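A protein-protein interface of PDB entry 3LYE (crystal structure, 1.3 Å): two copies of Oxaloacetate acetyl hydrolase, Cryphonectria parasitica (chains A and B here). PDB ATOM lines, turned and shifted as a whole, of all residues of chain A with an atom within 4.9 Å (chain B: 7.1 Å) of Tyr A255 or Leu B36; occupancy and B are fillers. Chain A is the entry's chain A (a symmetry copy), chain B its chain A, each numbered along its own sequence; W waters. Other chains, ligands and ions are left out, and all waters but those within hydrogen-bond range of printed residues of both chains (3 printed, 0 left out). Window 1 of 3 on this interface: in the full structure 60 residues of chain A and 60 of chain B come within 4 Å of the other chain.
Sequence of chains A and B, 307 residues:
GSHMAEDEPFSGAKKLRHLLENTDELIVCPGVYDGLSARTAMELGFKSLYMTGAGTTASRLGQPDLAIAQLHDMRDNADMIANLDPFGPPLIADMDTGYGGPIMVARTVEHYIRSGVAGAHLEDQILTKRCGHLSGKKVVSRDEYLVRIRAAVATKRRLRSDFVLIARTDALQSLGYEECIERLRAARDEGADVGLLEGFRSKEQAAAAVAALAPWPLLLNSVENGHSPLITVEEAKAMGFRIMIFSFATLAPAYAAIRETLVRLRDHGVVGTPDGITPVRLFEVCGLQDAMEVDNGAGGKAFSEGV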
ATOM      1  N   TYR A  33     -12.669   5.960 -16.947  1.00  0.00           N
ATOM      2  CA  TYR A  33     -11.862   5.607 -18.082  1.00  0.00           C
ATOM      3  C   TYR A  33     -12.540   5.588 -19.433  1.00  0.00           C
ATOM      4  O   TYR A  33     -11.889   5.309 -20.449  1.00  0.00           O
ATOM      5  CB  TYR A  33     -11.326   4.175 -17.848  1.00  0.00           C
ATOM      6  CG  TYR A  33     -12.368   3.102 -17.808  1.00  0.00           C
ATOM      7  CD1 TYR A  33     -12.765   2.462 -18.969  1.00  0.00           C
ATOM      8  CD2 TYR A  33     -12.970   2.728 -16.618  1.00  0.00           C
ATOM      9  CE1 TYR A  33     -13.726   1.489 -18.951  1.00  0.00           C
ATOM     10  CE2 TYR A  33     -13.939   1.734 -16.589  1.00  0.00           C
ATOM     11  CZ  TYR A  33     -14.325   1.118 -17.765  1.00  0.00           C
ATOM     12  OH  TYR A  33     -15.249   0.093 -17.715  1.00  0.00           O
ATOM     13  N   ALA A  58      -6.486   0.342 -21.206  1.00  0.00           N
ATOM     14  CA  ALA A  58      -7.224  -0.896 -21.271  1.00  0.00           C
ATOM     15  C   ALA A  58      -8.472  -0.771 -22.114  1.00  0.00           C
ATOM     16  O   ALA A  58      -8.776  -1.679 -22.912  1.00  0.00           O
ATOM     17  CB  ALA A  58      -7.606  -1.327 -19.872  1.00  0.00           C
ATOM     18  N   SER A  59      -9.209   0.312 -21.930  1.00  0.00           N
ATOM     19  CA  SER A  59     -10.468   0.471 -22.650  1.00  0.00           C
ATOM     20  C   SER A  59     -10.352   0.916 -24.094  1.00  0.00           C
ATOM     21  O   SER A  59     -10.974   0.316 -24.973  1.00  0.00           O
ATOM     22  CB  SER A  59     -11.352   1.403 -21.838  1.00  0.00           C
ATOM     23  OG  SER A  59     -12.640   1.596 -22.416  1.00  0.00           O
ATOM     24  N   LEU A 251     -12.710   0.548 -13.370  1.00  0.00           N
ATOM     25  CA  LEU A 251     -12.234  -0.499 -14.288  1.00  0.00           C
ATOM     26  C   LEU A 251     -12.309  -1.874 -13.643  1.00  0.00           C
ATOM     27  O   LEU A 251     -12.731  -2.847 -14.266  1.00  0.00           O
ATOM     28  CB  LEU A 251     -10.785  -0.200 -14.720  1.00  0.00           C
ATOM     29  CG  LEU A 251     -10.261  -1.018 -15.899  1.00  0.00           C
ATOM     30  CD1 LEU A 251     -10.827  -0.505 -17.198  1.00  0.00           C
ATOM     31  CD2 LEU A 251      -8.783  -0.950 -15.959  1.00  0.00           C
ATOM     32  N   ALA A 252     -11.918  -1.969 -12.373  1.00  0.00           N
ATOM     33  CA  ALA A 252     -11.928  -3.245 -11.621  1.00  0.00           C
ATOM     34  C   ALA A 252     -13.317  -3.862 -11.470  1.00  0.00           C
ATOM     35  O   ALA A 252     -13.519  -5.008 -11.875  1.00  0.00           O
ATOM     36  CB  ALA A 252     -11.188  -3.111 -10.282  1.00  0.00           C
ATOM     37  N   PRO A 253     -14.286  -3.122 -10.941  1.00  0.00           N
ATOM     38  CA  PRO A 253     -15.607  -3.757 -10.846  1.00  0.00           C
ATOM     39  C   PRO A 253     -16.210  -4.002 -12.222  1.00  0.00           C
ATOM     40  O   PRO A 253     -16.967  -4.957 -12.352  1.00  0.00           O
ATOM     41  CB  PRO A 253     -16.439  -2.745 -10.056  1.00  0.00           C
ATOM     42  CG  PRO A 253     -15.685  -1.413 -10.222  1.00  0.00           C
ATOM     43  CD  PRO A 253     -14.247  -1.817 -10.251  1.00  0.00           C
ATOM     44  N   ALA A 254     -15.916  -3.182 -13.226  1.00  0.00           N
ATOM     45  CA  ALA A 254     -16.478  -3.438 -14.553  1.00  0.00           C
ATOM     46  C   ALA A 254     -15.955  -4.816 -15.008  1.00  0.00           C
ATOM     47  O   ALA A 254     -16.721  -5.633 -15.514  1.00  0.00           O
ATOM     48  CB  ALA A 254     -16.040  -2.362 -15.513  1.00  0.00           C
ATOM     49  N   TYR A 255     -14.656  -5.064 -14.869  1.00  0.00           N
ATOM     50  CA  TYR A 255     -14.115  -6.342 -15.281  1.00  0.00           C
ATOM     51  C   TYR A 255     -14.771  -7.502 -14.551  1.00  0.00           C
ATOM     52  O   TYR A 255     -15.164  -8.480 -15.159  1.00  0.00           O
ATOM     53  CB  TYR A 255     -12.605  -6.443 -14.990  1.00  0.00           C
ATOM     54  CG  TYR A 255     -12.066  -7.849 -15.162  1.00  0.00           C
ATOM     55  CD1 TYR A 255     -11.976  -8.427 -16.406  1.00  0.00           C
ATOM     56  CD2 TYR A 255     -11.707  -8.616 -14.075  1.00  0.00           C
ATOM     57  CE1 TYR A 255     -11.514  -9.689 -16.567  1.00  0.00           C
ATOM     58  CE2 TYR A 255     -11.239  -9.914 -14.230  1.00  0.00           C
ATOM     59  CZ  TYR A 255     -11.144 -10.435 -15.477  1.00  0.00           C
ATOM     60  OH  TYR A 255     -10.699 -11.722 -15.652  1.00  0.00           O
ATOM     61  N   ALA A 256     -14.867  -7.418 -13.236  1.00  0.00           N
ATOM     62  CA  ALA A 256     -15.454  -8.521 -12.496  1.00  0.00           C
ATOM     63  C   ALA A 256     -16.865  -8.856 -12.941  1.00  0.00           C
ATOM     64  O   ALA A 256     -17.244 -10.040 -13.020  1.00  0.00           O
ATOM     65  CB  ALA A 256     -15.429  -8.223 -11.025  1.00  0.00           C
ATOM     66  N   ALA A 257     -17.650  -7.816 -13.202  1.00  0.00           N
ATOM     67  CA  ALA A 257     -19.039  -7.975 -13.624  1.00  0.00           C
ATOM     68  C   ALA A 257     -19.139  -8.529 -15.053  1.00  0.00           C
ATOM     69  O   ALA A 257     -19.991  -9.408 -15.324  1.00  0.00           O
ATOM     70  CB  ALA A 257     -19.770  -6.656 -13.516  1.00  0.00           C
ATOM     71  N   ILE A 258     -18.353  -7.962 -15.972  1.00  0.00           N
ATOM     72  CA  ILE A 258     -18.332  -8.433 -17.333  1.00  0.00           C
ATOM     73  C   ILE A 258     -17.931  -9.929 -17.340  1.00  0.00           C
ATOM     74  O   ILE A 258     -18.545 -10.762 -18.020  1.00  0.00           O
ATOM     75  CB  ILE A 258     -17.345  -7.604 -18.164  1.00  0.00           C
ATOM     76  CG1 ILE A 258     -17.896  -6.208 -18.333  1.00  0.00           C
ATOM     77  CG2 ILE A 258     -17.032  -8.298 -19.482  1.00  0.00           C
ATOM     78  CD1 ILE A 258     -16.877  -5.218 -18.902  1.00  0.00           C
ATOM     79  N   ARG A 259     -16.927 -10.289 -16.549  1.00  0.00           N
ATOM     80  CA  ARG A 259     -16.476 -11.673 -16.502  1.00  0.00           C
ATOM     81  C   ARG A 259     -17.536 -12.634 -15.985  1.00  0.00           C
ATOM     82  O   ARG A 259     -17.808 -13.669 -16.580  1.00  0.00           O
ATOM     83  CB  ARG A 259     -15.221 -11.807 -15.676  1.00  0.00           C
ATOM     84  CG  ARG A 259     -14.523 -13.122 -15.853  1.00  0.00           C
ATOM     85  CD  ARG A 259     -13.440 -13.314 -14.850  1.00  0.00           C
ATOM     86  NE  ARG A 259     -12.491 -14.319 -15.325  1.00  0.00           N
ATOM     87  CZ  ARG A 259     -12.708 -15.638 -15.308  1.00  0.00           C
ATOM     88  NH1 ARG A 259     -11.785 -16.436 -15.790  1.00  0.00           N
ATOM     89  NH2 ARG A 259     -13.832 -16.162 -14.828  1.00  0.00           N
ATOM     90  N   GLU A 260     -18.143 -12.275 -14.865  1.00  0.00           N
ATOM     91  CA  GLU A 260     -19.180 -13.138 -14.282  1.00  0.00           C
ATOM     92  C   GLU A 260     -20.350 -13.296 -15.249  1.00  0.00           C
ATOM     93  O   GLU A 260     -20.928 -14.376 -15.385  1.00  0.00           O
ATOM     94  CB  GLU A 260     -19.686 -12.544 -12.957  1.00  0.00           C
ATOM     95  CG  GLU A 260     -20.742 -13.376 -12.256  1.00  0.00           C
ATOM     96  CD  GLU A 260     -20.822 -13.090 -10.764  1.00  0.00           C
ATOM     97  OE1 GLU A 260     -20.338 -12.019 -10.344  1.00  0.00           O
ATOM     98  OE2 GLU A 260     -21.366 -13.958 -10.028  1.00  0.00           O
ATOM     99  N   VAL B  32     -19.484  -6.786 -27.174  1.00  0.00           N
ATOM    100  CA  VAL B  32     -18.359  -6.109 -26.570  1.00  0.00           C
ATOM    101  C   VAL B  32     -18.331  -4.684 -27.102  1.00  0.00           C
ATOM    102  O   VAL B  32     -18.835  -4.405 -28.172  1.00  0.00           O
ATOM    103  CB  VAL B  32     -17.044  -6.871 -26.730  1.00  0.00           C
ATOM    104  CG1 VAL B  32     -17.146  -8.262 -26.126  1.00  0.00           C
ATOM    105  CG2 VAL B  32     -16.643  -6.949 -28.164  1.00  0.00           C
ATOM    106  N   TYR B  33     -17.657  -3.804 -26.377  1.00  0.00           N
ATOM    107  CA  TYR B  33     -17.658  -2.415 -26.742  1.00  0.00           C
ATOM    108  C   TYR B  33     -16.387  -1.634 -26.493  1.00  0.00           C
ATOM    109  O   TYR B  33     -16.324  -0.438 -26.805  1.00  0.00           O
ATOM    110  CB  TYR B  33     -18.763  -1.715 -25.917  1.00  0.00           C
ATOM    111  CG  TYR B  33     -18.538  -1.692 -24.437  1.00  0.00           C
ATOM    112  CD1 TYR B  33     -17.833  -0.656 -23.849  1.00  0.00           C
ATOM    113  CD2 TYR B  33     -19.014  -2.704 -23.622  1.00  0.00           C
ATOM    114  CE1 TYR B  33     -17.607  -0.628 -22.500  1.00  0.00           C
ATOM    115  CE2 TYR B  33     -18.798  -2.678 -22.251  1.00  0.00           C
ATOM    116  CZ  TYR B  33     -18.081  -1.637 -21.689  1.00  0.00           C
ATOM    117  OH  TYR B  33     -17.921  -1.595 -20.318  1.00  0.00           O
ATOM    118  N   ASP B  34     -15.368  -2.295 -25.963  1.00  0.00           N
ATOM    119  CA  ASP B  34     -14.098  -1.658 -25.649  1.00  0.00           C
ATOM    120  C   ASP B  34     -13.048  -2.727 -25.472  1.00  0.00           C
ATOM    121  O   ASP B  34     -13.339  -3.935 -25.660  1.00  0.00           O
ATOM    122  CB  ASP B  34     -14.200  -0.726 -24.442  1.00  0.00           C
ATOM    123  CG  ASP B  34     -14.208  -1.455 -23.101  1.00  0.00           C
ATOM    124  OD1 ASP B  34     -13.803  -0.820 -22.094  1.00  0.00           O
ATOM    125  OD2 ASP B  34     -14.631  -2.639 -23.051  1.00  0.00           O
ATOM    126  N   GLY B  35     -11.850  -2.325 -25.093  1.00  0.00           N
ATOM    127  CA  GLY B  35     -10.780  -3.281 -24.966  1.00  0.00           C
ATOM    128  C   GLY B  35     -10.939  -4.244 -23.807  1.00  0.00           C
ATOM    129  O   GLY B  35     -10.669  -5.425 -23.944  1.00  0.00           O
ATOM    130  N   LEU B  36     -11.441  -3.747 -22.687  1.00  0.00           N
ATOM    131  CA  LEU B  36     -11.625  -4.588 -21.527  1.00  0.00           C
ATOM    132  C   LEU B  36     -12.690  -5.650 -21.773  1.00  0.00           C
ATOM    133  O   LEU B  36     -12.484  -6.827 -21.507  1.00  0.00           O
ATOM    134  CB  LEU B  36     -11.977  -3.740 -20.326  1.00  0.00           C
ATOM    135  CG  LEU B  36     -12.151  -4.515 -19.024  1.00  0.00           C
ATOM    136  CD1 LEU B  36     -10.832  -5.204 -18.578  1.00  0.00           C
ATOM    137  CD2 LEU B  36     -12.704  -3.661 -17.934  1.00  0.00           C
ATOM    138  N   SER B  37     -13.845  -5.237 -22.268  1.00  0.00           N
ATOM    139  CA  SER B  37     -14.912  -6.193 -22.535  1.00  0.00           C
ATOM    140  C   SER B  37     -14.452  -7.219 -23.591  1.00  0.00           C
ATOM    141  O   SER B  37     -14.680  -8.425 -23.447  1.00  0.00           O
ATOM    142  CB  SER B  37     -16.214  -5.517 -22.973  1.00  0.00           C
ATOM    143  OG  SER B  37     -16.008  -4.660 -24.072  1.00  0.00           O
ATOM    144  N   ALA B  38     -13.784  -6.769 -24.640  1.00  0.00           N
ATOM    145  CA  ALA B  38     -13.304  -7.692 -25.655  1.00  0.00           C
ATOM    146  C   ALA B  38     -12.257  -8.665 -25.102  1.00  0.00           C
ATOM    147  O   ALA B  38     -12.308  -9.879 -25.355  1.00  0.00           O
ATOM    148  CB  ALA B  38     -12.731  -6.927 -26.835  1.00  0.00           C
ATOM    149  N   ARG B  39     -11.310  -8.146 -24.328  1.00  0.00           N
ATOM    150  CA  ARG B  39     -10.271  -9.004 -23.752  1.00  0.00           C
ATOM    151  C   ARG B  39     -10.881 -10.039 -22.800  1.00  0.00           C
ATOM    152  O   ARG B  39     -10.391 -11.154 -22.701  1.00  0.00           O
ATOM    153  CB  ARG B  39      -9.247  -8.151 -23.004  1.00  0.00           C
ATOM    154  CG  ARG B  39      -8.264  -7.408 -23.892  1.00  0.00           C
ATOM    155  CD  ARG B  39      -7.276  -8.324 -24.592  1.00  0.00           C
ATOM    156  NE  ARG B  39      -6.158  -7.532 -25.083  1.00  0.00           N
ATOM    157  CZ  ARG B  39      -5.098  -8.034 -25.695  1.00  0.00           C
ATOM    158  NH1 ARG B  39      -4.143  -7.212 -26.075  1.00  0.00           N
ATOM    159  NH2 ARG B  39      -5.009  -9.337 -25.924  1.00  0.00           N
ATOM    160  N   THR B  40     -11.946  -9.655 -22.111  1.00  0.00           N
ATOM    161  CA  THR B  40     -12.588 -10.583 -21.177  1.00  0.00           C
ATOM    162  C   THR B  40     -13.266 -11.722 -21.957  1.00  0.00           C
ATOM    163  O   THR B  40     -13.169 -12.898 -21.608  1.00  0.00           O
ATOM    164  CB  THR B  40     -13.564  -9.893 -20.240  1.00  0.00           C
ATOM    165  OG1 THR B  40     -12.885  -8.853 -19.531  1.00  0.00           O
ATOM    166  CG2 THR B  40     -14.098 -10.824 -19.190  1.00  0.00           C
ATOM    167  N   ALA B  41     -13.966 -11.381 -23.026  1.00  0.00           N
ATOM    168  CA  ALA B  41     -14.602 -12.398 -23.863  1.00  0.00           C
ATOM    169  C   ALA B  41     -13.540 -13.342 -24.432  1.00  0.00           C
ATOM    170  O   ALA B  41     -13.755 -14.540 -24.554  1.00  0.00           O
ATOM    171  CB  ALA B  41     -15.391 -11.751 -24.959  1.00  0.00           C
ATOM    172  N   MET B  42     -12.379 -12.790 -24.785  1.00  0.00           N
ATOM    173  CA  MET B  42     -11.263 -13.581 -25.321  1.00  0.00           C
ATOM    174  C   MET B  42     -10.712 -14.522 -24.250  1.00  0.00           C
ATOM    175  O   MET B  42     -10.484 -15.693 -24.522  1.00  0.00           O
ATOM    176  CB  MET B  42     -10.147 -12.677 -25.846  1.00  0.00           C
ATOM    177  CG  MET B  42     -10.564 -11.880 -27.062  1.00  0.00           C
ATOM    178  SD  MET B  42      -9.527 -10.432 -27.438  1.00  0.00           S
ATOM    179  CE  MET B  42      -8.039 -11.189 -28.016  1.00  0.00           C
ATOM    180  N   GLU B  43     -10.537 -14.012 -23.038  1.00  0.00           N
ATOM    181  CA  GLU B  43     -10.031 -14.793 -21.917  1.00  0.00           C
ATOM    182  C   GLU B  43     -10.922 -16.017 -21.691  1.00  0.00           C
ATOM    183  O   GLU B  43     -10.436 -17.116 -21.398  1.00  0.00           O
ATOM    184  CB  GLU B  43     -10.124 -13.950 -20.614  1.00  0.00           C
ATOM    185  CG  GLU B  43      -9.829 -14.678 -19.305  1.00  0.00           C
ATOM    186  CD  GLU B  43     -10.128 -13.875 -18.027  1.00  0.00           C
ATOM    187  OE1 GLU B  43      -9.837 -14.413 -16.926  1.00  0.00           O
ATOM    188  OE2 GLU B  43     -10.626 -12.744 -18.077  1.00  0.00           O
ATOM    189  N   LEU B  44     -12.221 -15.835 -21.892  1.00  0.00           N
ATOM    190  CA  LEU B  44     -13.198 -16.894 -21.651  1.00  0.00           C
ATOM    191  C   LEU B  44     -13.384 -17.854 -22.794  1.00  0.00           C
ATOM    192  O   LEU B  44     -14.141 -18.813 -22.680  1.00  0.00           O
ATOM    193  CB  LEU B  44     -14.528 -16.279 -21.183  1.00  0.00           C
ATOM    194  CG  LEU B  44     -14.427 -15.504 -19.857  1.00  0.00           C
ATOM    195  CD1 LEU B  44     -15.699 -14.702 -19.607  1.00  0.00           C
ATOM    196  CD2 LEU B  44     -14.095 -16.419 -18.684  1.00  0.00           C
ATOM    197  N   MET B  80      -9.400  -1.784 -33.395  1.00  0.00           N
ATOM    198  CA  MET B  80      -8.771  -2.083 -32.136  1.00  0.00           C
ATOM    199  C   MET B  80      -9.175  -3.479 -31.634  1.00  0.00           C
ATOM    200  O   MET B  80      -8.325  -4.313 -31.304  1.00  0.00           O
ATOM    201  CB  MET B  80      -9.114  -1.007 -31.085  1.00  0.00           C
ATOM    202  CG  MET B  80      -8.466  -1.226 -29.729  1.00  0.00           C
ATOM    203  SD  MET B  80      -9.438  -2.282 -28.580  1.00  0.00           S
ATOM    204  CE  MET B  80     -10.883  -1.251 -28.274  1.00  0.00           C
ATOM    205  N   LEU B  84      -6.630  -7.315 -31.382  1.00  0.00           N
ATOM    206  CA  LEU B  84      -6.005  -7.502 -30.075  1.00  0.00           C
ATOM    207  C   LEU B  84      -5.125  -8.760 -30.151  1.00  0.00           C
ATOM    208  O   LEU B  84      -4.038  -8.786 -29.582  1.00  0.00           O
ATOM    209  CB  LEU B  84      -7.034  -7.556 -28.967  1.00  0.00           C
ATOM    210  CG  LEU B  84      -7.761  -6.251 -28.713  1.00  0.00           C
ATOM    211  CD1 LEU B  84      -8.853  -6.456 -27.690  1.00  0.00           C
ATOM    212  CD2 LEU B  84      -6.776  -5.151 -28.297  1.00  0.00           C
ATOM    213  N   ALA B 254     -21.582  -3.883 -16.756  1.00  0.00           N
ATOM    214  CA  ALA B 254     -20.504  -2.964 -16.390  1.00  0.00           C
ATOM    215  C   ALA B 254     -21.158  -1.755 -15.690  1.00  0.00           C
ATOM    216  O   ALA B 254     -20.679  -1.306 -14.652  1.00  0.00           O
ATOM    217  CB  ALA B 254     -19.762  -2.522 -17.625  1.00  0.00           C
ATOM    218  N   ALA B 257     -22.379  -2.503 -12.072  1.00  0.00           N
ATOM    219  CA  ALA B 257     -21.254  -2.684 -11.159  1.00  0.00           C
ATOM    220  C   ALA B 257     -20.550  -1.354 -10.853  1.00  0.00           C
ATOM    221  O   ALA B 257     -20.183  -1.097  -9.683  1.00  0.00           O
ATOM    222  CB  ALA B 257     -20.273  -3.682 -11.732  1.00  0.00           C
ATOM    223  N   ILE B 258     -20.282  -0.564 -11.896  1.00  0.00           N
ATOM    224  CA  ILE B 258     -19.666   0.725 -11.721  1.00  0.00           C
ATOM    225  C   ILE B 258     -20.561   1.586 -10.795  1.00  0.00           C
ATOM    226  O   ILE B 258     -20.084   2.243  -9.859  1.00  0.00           O
ATOM    227  CB  ILE B 258     -19.475   1.410 -13.080  1.00  0.00           C
ATOM    228  CG1 ILE B 258     -18.414   0.669 -13.859  1.00  0.00           C
ATOM    229  CG2 ILE B 258     -19.176   2.892 -12.901  1.00  0.00           C
ATOM    230  CD1 ILE B 258     -18.337   1.088 -15.329  1.00  0.00           C
ATOM    231  N   GLY B 276      -9.054  -9.950  -5.368  1.00  0.00           N
ATOM    232  CA  GLY B 276      -8.335 -10.626  -6.429  1.00  0.00           C
ATOM    233  C   GLY B 276      -8.353  -9.861  -7.741  1.00  0.00           C
ATOM    234  O   GLY B 276      -7.641 -10.253  -8.649  1.00  0.00           O
ATOM    235  N   ILE B 277      -9.129  -8.776  -7.835  1.00  0.00           N
ATOM    236  CA  ILE B 277      -9.176  -8.007  -9.094  1.00  0.00           C
ATOM    237  C   ILE B 277      -8.108  -6.920  -8.964  1.00  0.00           C
ATOM    238  O   ILE B 277      -8.397  -5.744  -8.692  1.00  0.00           O
ATOM    239  CB  ILE B 277     -10.531  -7.403  -9.350  1.00  0.00           C
ATOM    240  CG1 ILE B 277     -11.671  -8.429  -9.165  1.00  0.00           C
ATOM    241  CG2 ILE B 277     -10.524  -6.822 -10.757  1.00  0.00           C
ATOM    242  CD1 ILE B 277     -11.532  -9.698  -9.979  1.00  0.00           C
ATOM    243  N   THR B 278      -6.864  -7.350  -9.093  1.00  0.00           N
ATOM    244  CA  THR B 278      -5.682  -6.489  -8.971  1.00  0.00           C
ATOM    245  C   THR B 278      -5.277  -5.834 -10.278  1.00  0.00           C
ATOM    246  O   THR B 278      -5.698  -6.259 -11.346  1.00  0.00           O
ATOM    247  CB  THR B 278      -4.467  -7.336  -8.524  1.00  0.00           C
ATOM    248  OG1 THR B 278      -4.269  -8.345  -9.521  1.00  0.00           O
ATOM    249  CG2 THR B 278      -4.671  -7.988  -7.121  1.00  0.00           C
ATOM    250  N   ARG B 281      -3.809  -8.406 -12.493  1.00  0.00           N
ATOM    251  CA  ARG B 281      -4.740  -9.316 -13.143  1.00  0.00           C
ATOM    252  C   ARG B 281      -5.377  -8.607 -14.348  1.00  0.00           C
ATOM    253  O   ARG B 281      -5.553  -9.194 -15.393  1.00  0.00           O
ATOM    254  CB  ARG B 281      -5.847  -9.763 -12.202  1.00  0.00           C
ATOM    255  CG  ARG B 281      -6.814 -10.753 -12.852  1.00  0.00           C
ATOM    256  CD  ARG B 281      -7.724 -11.432 -11.902  1.00  0.00           C
ATOM    257  NE  ARG B 281      -8.780 -12.129 -12.643  1.00  0.00           N
ATOM    258  CZ  ARG B 281      -9.801 -12.729 -12.054  1.00  0.00           C
ATOM    259  NH1 ARG B 281      -9.885 -12.741 -10.727  1.00  0.00           N
ATOM    260  NH2 ARG B 281     -10.720 -13.314 -12.781  1.00  0.00           N
ATOM    261  N   LEU B 282      -5.756  -7.340 -14.185  1.00  0.00           N
ATOM    262  CA  LEU B 282      -6.354  -6.580 -15.283  1.00  0.00           C
ATOM    263  C   LEU B 282      -5.347  -6.452 -16.441  1.00  0.00           C
ATOM    264  O   LEU B 282      -5.711  -6.575 -17.607  1.00  0.00           O
ATOM    265  CB  LEU B 282      -6.773  -5.208 -14.770  1.00  0.00           C
ATOM    266  CG  LEU B 282      -7.940  -5.261 -13.780  1.00  0.00           C
ATOM    267  CD1 LEU B 282      -8.047  -3.924 -13.019  1.00  0.00           C
ATOM    268  CD2 LEU B 282      -9.236  -5.684 -14.487  1.00  0.00           C
ATOM    269  N   VAL B 285      -5.230  -9.689 -18.305  1.00  0.00           N
ATOM    270  CA  VAL B 285      -6.397  -9.867 -19.163  1.00  0.00           C
ATOM    271  C   VAL B 285      -6.179  -9.031 -20.423  1.00  0.00           C
ATOM    272  O   VAL B 285      -6.492  -9.442 -21.529  1.00  0.00           O
ATOM    273  CB  VAL B 285      -7.682  -9.404 -18.426  1.00  0.00           C
ATOM    274  CG1 VAL B 285      -8.867  -9.176 -19.385  1.00  0.00           C
ATOM    275  CG2 VAL B 285      -8.030 -10.368 -17.276  1.00  0.00           C
ATOM    276  N   CYS B 286      -5.553  -7.878 -20.260  1.00  0.00           N
ATOM    277  CA  CYS B 286      -5.299  -6.965 -21.357  1.00  0.00           C
ATOM    278  C   CYS B 286      -3.985  -7.131 -22.110  1.00  0.00           C
ATOM    279  O   CYS B 286      -3.460  -6.154 -22.643  1.00  0.00           O
ATOM    280  CB  CYS B 286      -5.543  -5.514 -20.909  1.00  0.00           C
ATOM    281  SG  CYS B 286      -7.260  -5.162 -20.464  1.00  0.00           S
HETATM  282  O   HOH W   1      -8.031 -13.479 -15.142  1.00  0.00           O
HETATM  283  O   HOH W   2     -17.502   0.849 -19.307  1.00  0.00           O
HETATM  284  O   HOH W   3     -15.119  -1.643 -19.749  1.00  0.00           O
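Tyr A255 touches seven residues of chain B. Of the printed residues of chain A, Leu B36 touches Ala A58, Leu A251 and Tyr A255. Printed residues of chain B within 4 Å of Ala A257: Ala B257 (3.5 Å). Of the printed residues of chain A, Thr B40 touches Tyr A255, Ile A258 and Arg A259. Ile B258 touches none of the printed residues of chain A. The nearest residue of chain B that does not touch Tyr A255 is Arg B39 (6.3 Å). The nearest printed residue of chain A that does not touch Ile B277 is Ala A256 (4.2 Å).
Of the 13 printed residues of chain A, 10 touch a printed residue of chain B. Hydrophobic or aromatic side chains of chain A that line the printed part of chain B: Tyr A33, Ala A58, Leu A251, Ala A252, Tyr A255, Ala A257 and Ile A258. Of the 25 printed residues of chain B, 13 touch a printed residue of chain A. Hydrophobic or aromatic side chains of chain B within 4 Å of the printed part of chain A: Leu B36, Leu B44, Met B80, Ala B257, Ile B277, Leu B282 and Val B285. Among the printed residues, 23 pairs touch across the chains.
OG of Ser A59 lies within hydrogen-bond range of OD1 of Asp B34 (2.7 Å). N of Gly B35 is in hydrogen-bond range of O of Ser A59 (2.8 Å). O of Ala A58 sits at hydrogen-bond distance from N of Leu B36 (3.4 Å). The side-chain hydroxyl of Tyr A255 is in hydrogen-bond range of the side-chain carboxylate of Glu B43 (2.6 Å). OE1 of Glu B43 is in salt-bridge range of NH1 of Arg A259 (3.0 Å). The guanidinium group of Arg B281 is in hydrogen-bond range of the side-chain hydroxyl of Tyr A255. NE of Arg A259 lies close to NH2 of Arg B281, at 3.3 Å.
Ala A257 touches its own counterpart, Ala B257. Of the 23 pairs that touch across the chains among the printed residues, 1 has its exchanged pair printed and touching as well.
Water W2 bridges OH of Tyr B33 (2.7 Å) and OH of Tyr A33 (2.9 Å). Water W3 lies within hydrogen-bond range of the side-chain hydroxyl (OH) of Tyr A33 (2.7 Å), the side-chain carboxylate (OD1) of Asp B34 (2.8 Å) and the side-chain hydroxyl (OH) of Tyr B33 (2.9 Å). Water W1 lies within hydrogen-bond range of OE1 of Glu B43, NE of Arg B281 and OH of Tyr A255.
N of Leu B36 lies close to OD2 of Asp B34. OD2 of Asp B34 is in hydrogen-bond range of OG of Ser B37, at 2.7 Å. The backbone carbonyl oxygen (O) of Leu B36 is in hydrogen-bond range of the side-chain hydroxyl (OG1) of Thr B40 (2.9 Å). The backbone NH of Arg B281 is in hydrogen-bond range of the side-chain hydroxyl of Thr B278, 3.0 Å away. The side-chain sulfur (SG) of Cys B286 sits close to the backbone carbonyl oxygen (O) of Leu B282 (3.5 Å). The guanidinium group (NE) of Arg A259 is in hydrogen-bond range of the side-chain hydroxyl (OH) of Tyr A255.
Among the printed residues, merely in contact across the chains: Tyr A255 with Thr B40, Ala A58 with Gly B35, Tyr A255 with Val B285, Tyr A255 with Leu B282, Ala A257 with Ala B257, Pro A253 with Ala B257, Ser A59 with Met B80, Ala A252 with Ile B277, Arg A259 with Thr B40, Arg A259 with Leu B44, Leu A251 with Leu B36, Ile A258 with Thr B40, Tyr A255 with Leu B36, Ala A58 with Cys B286, Tyr A33 with Asp B34 and Tyr A255 with Ile B277.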
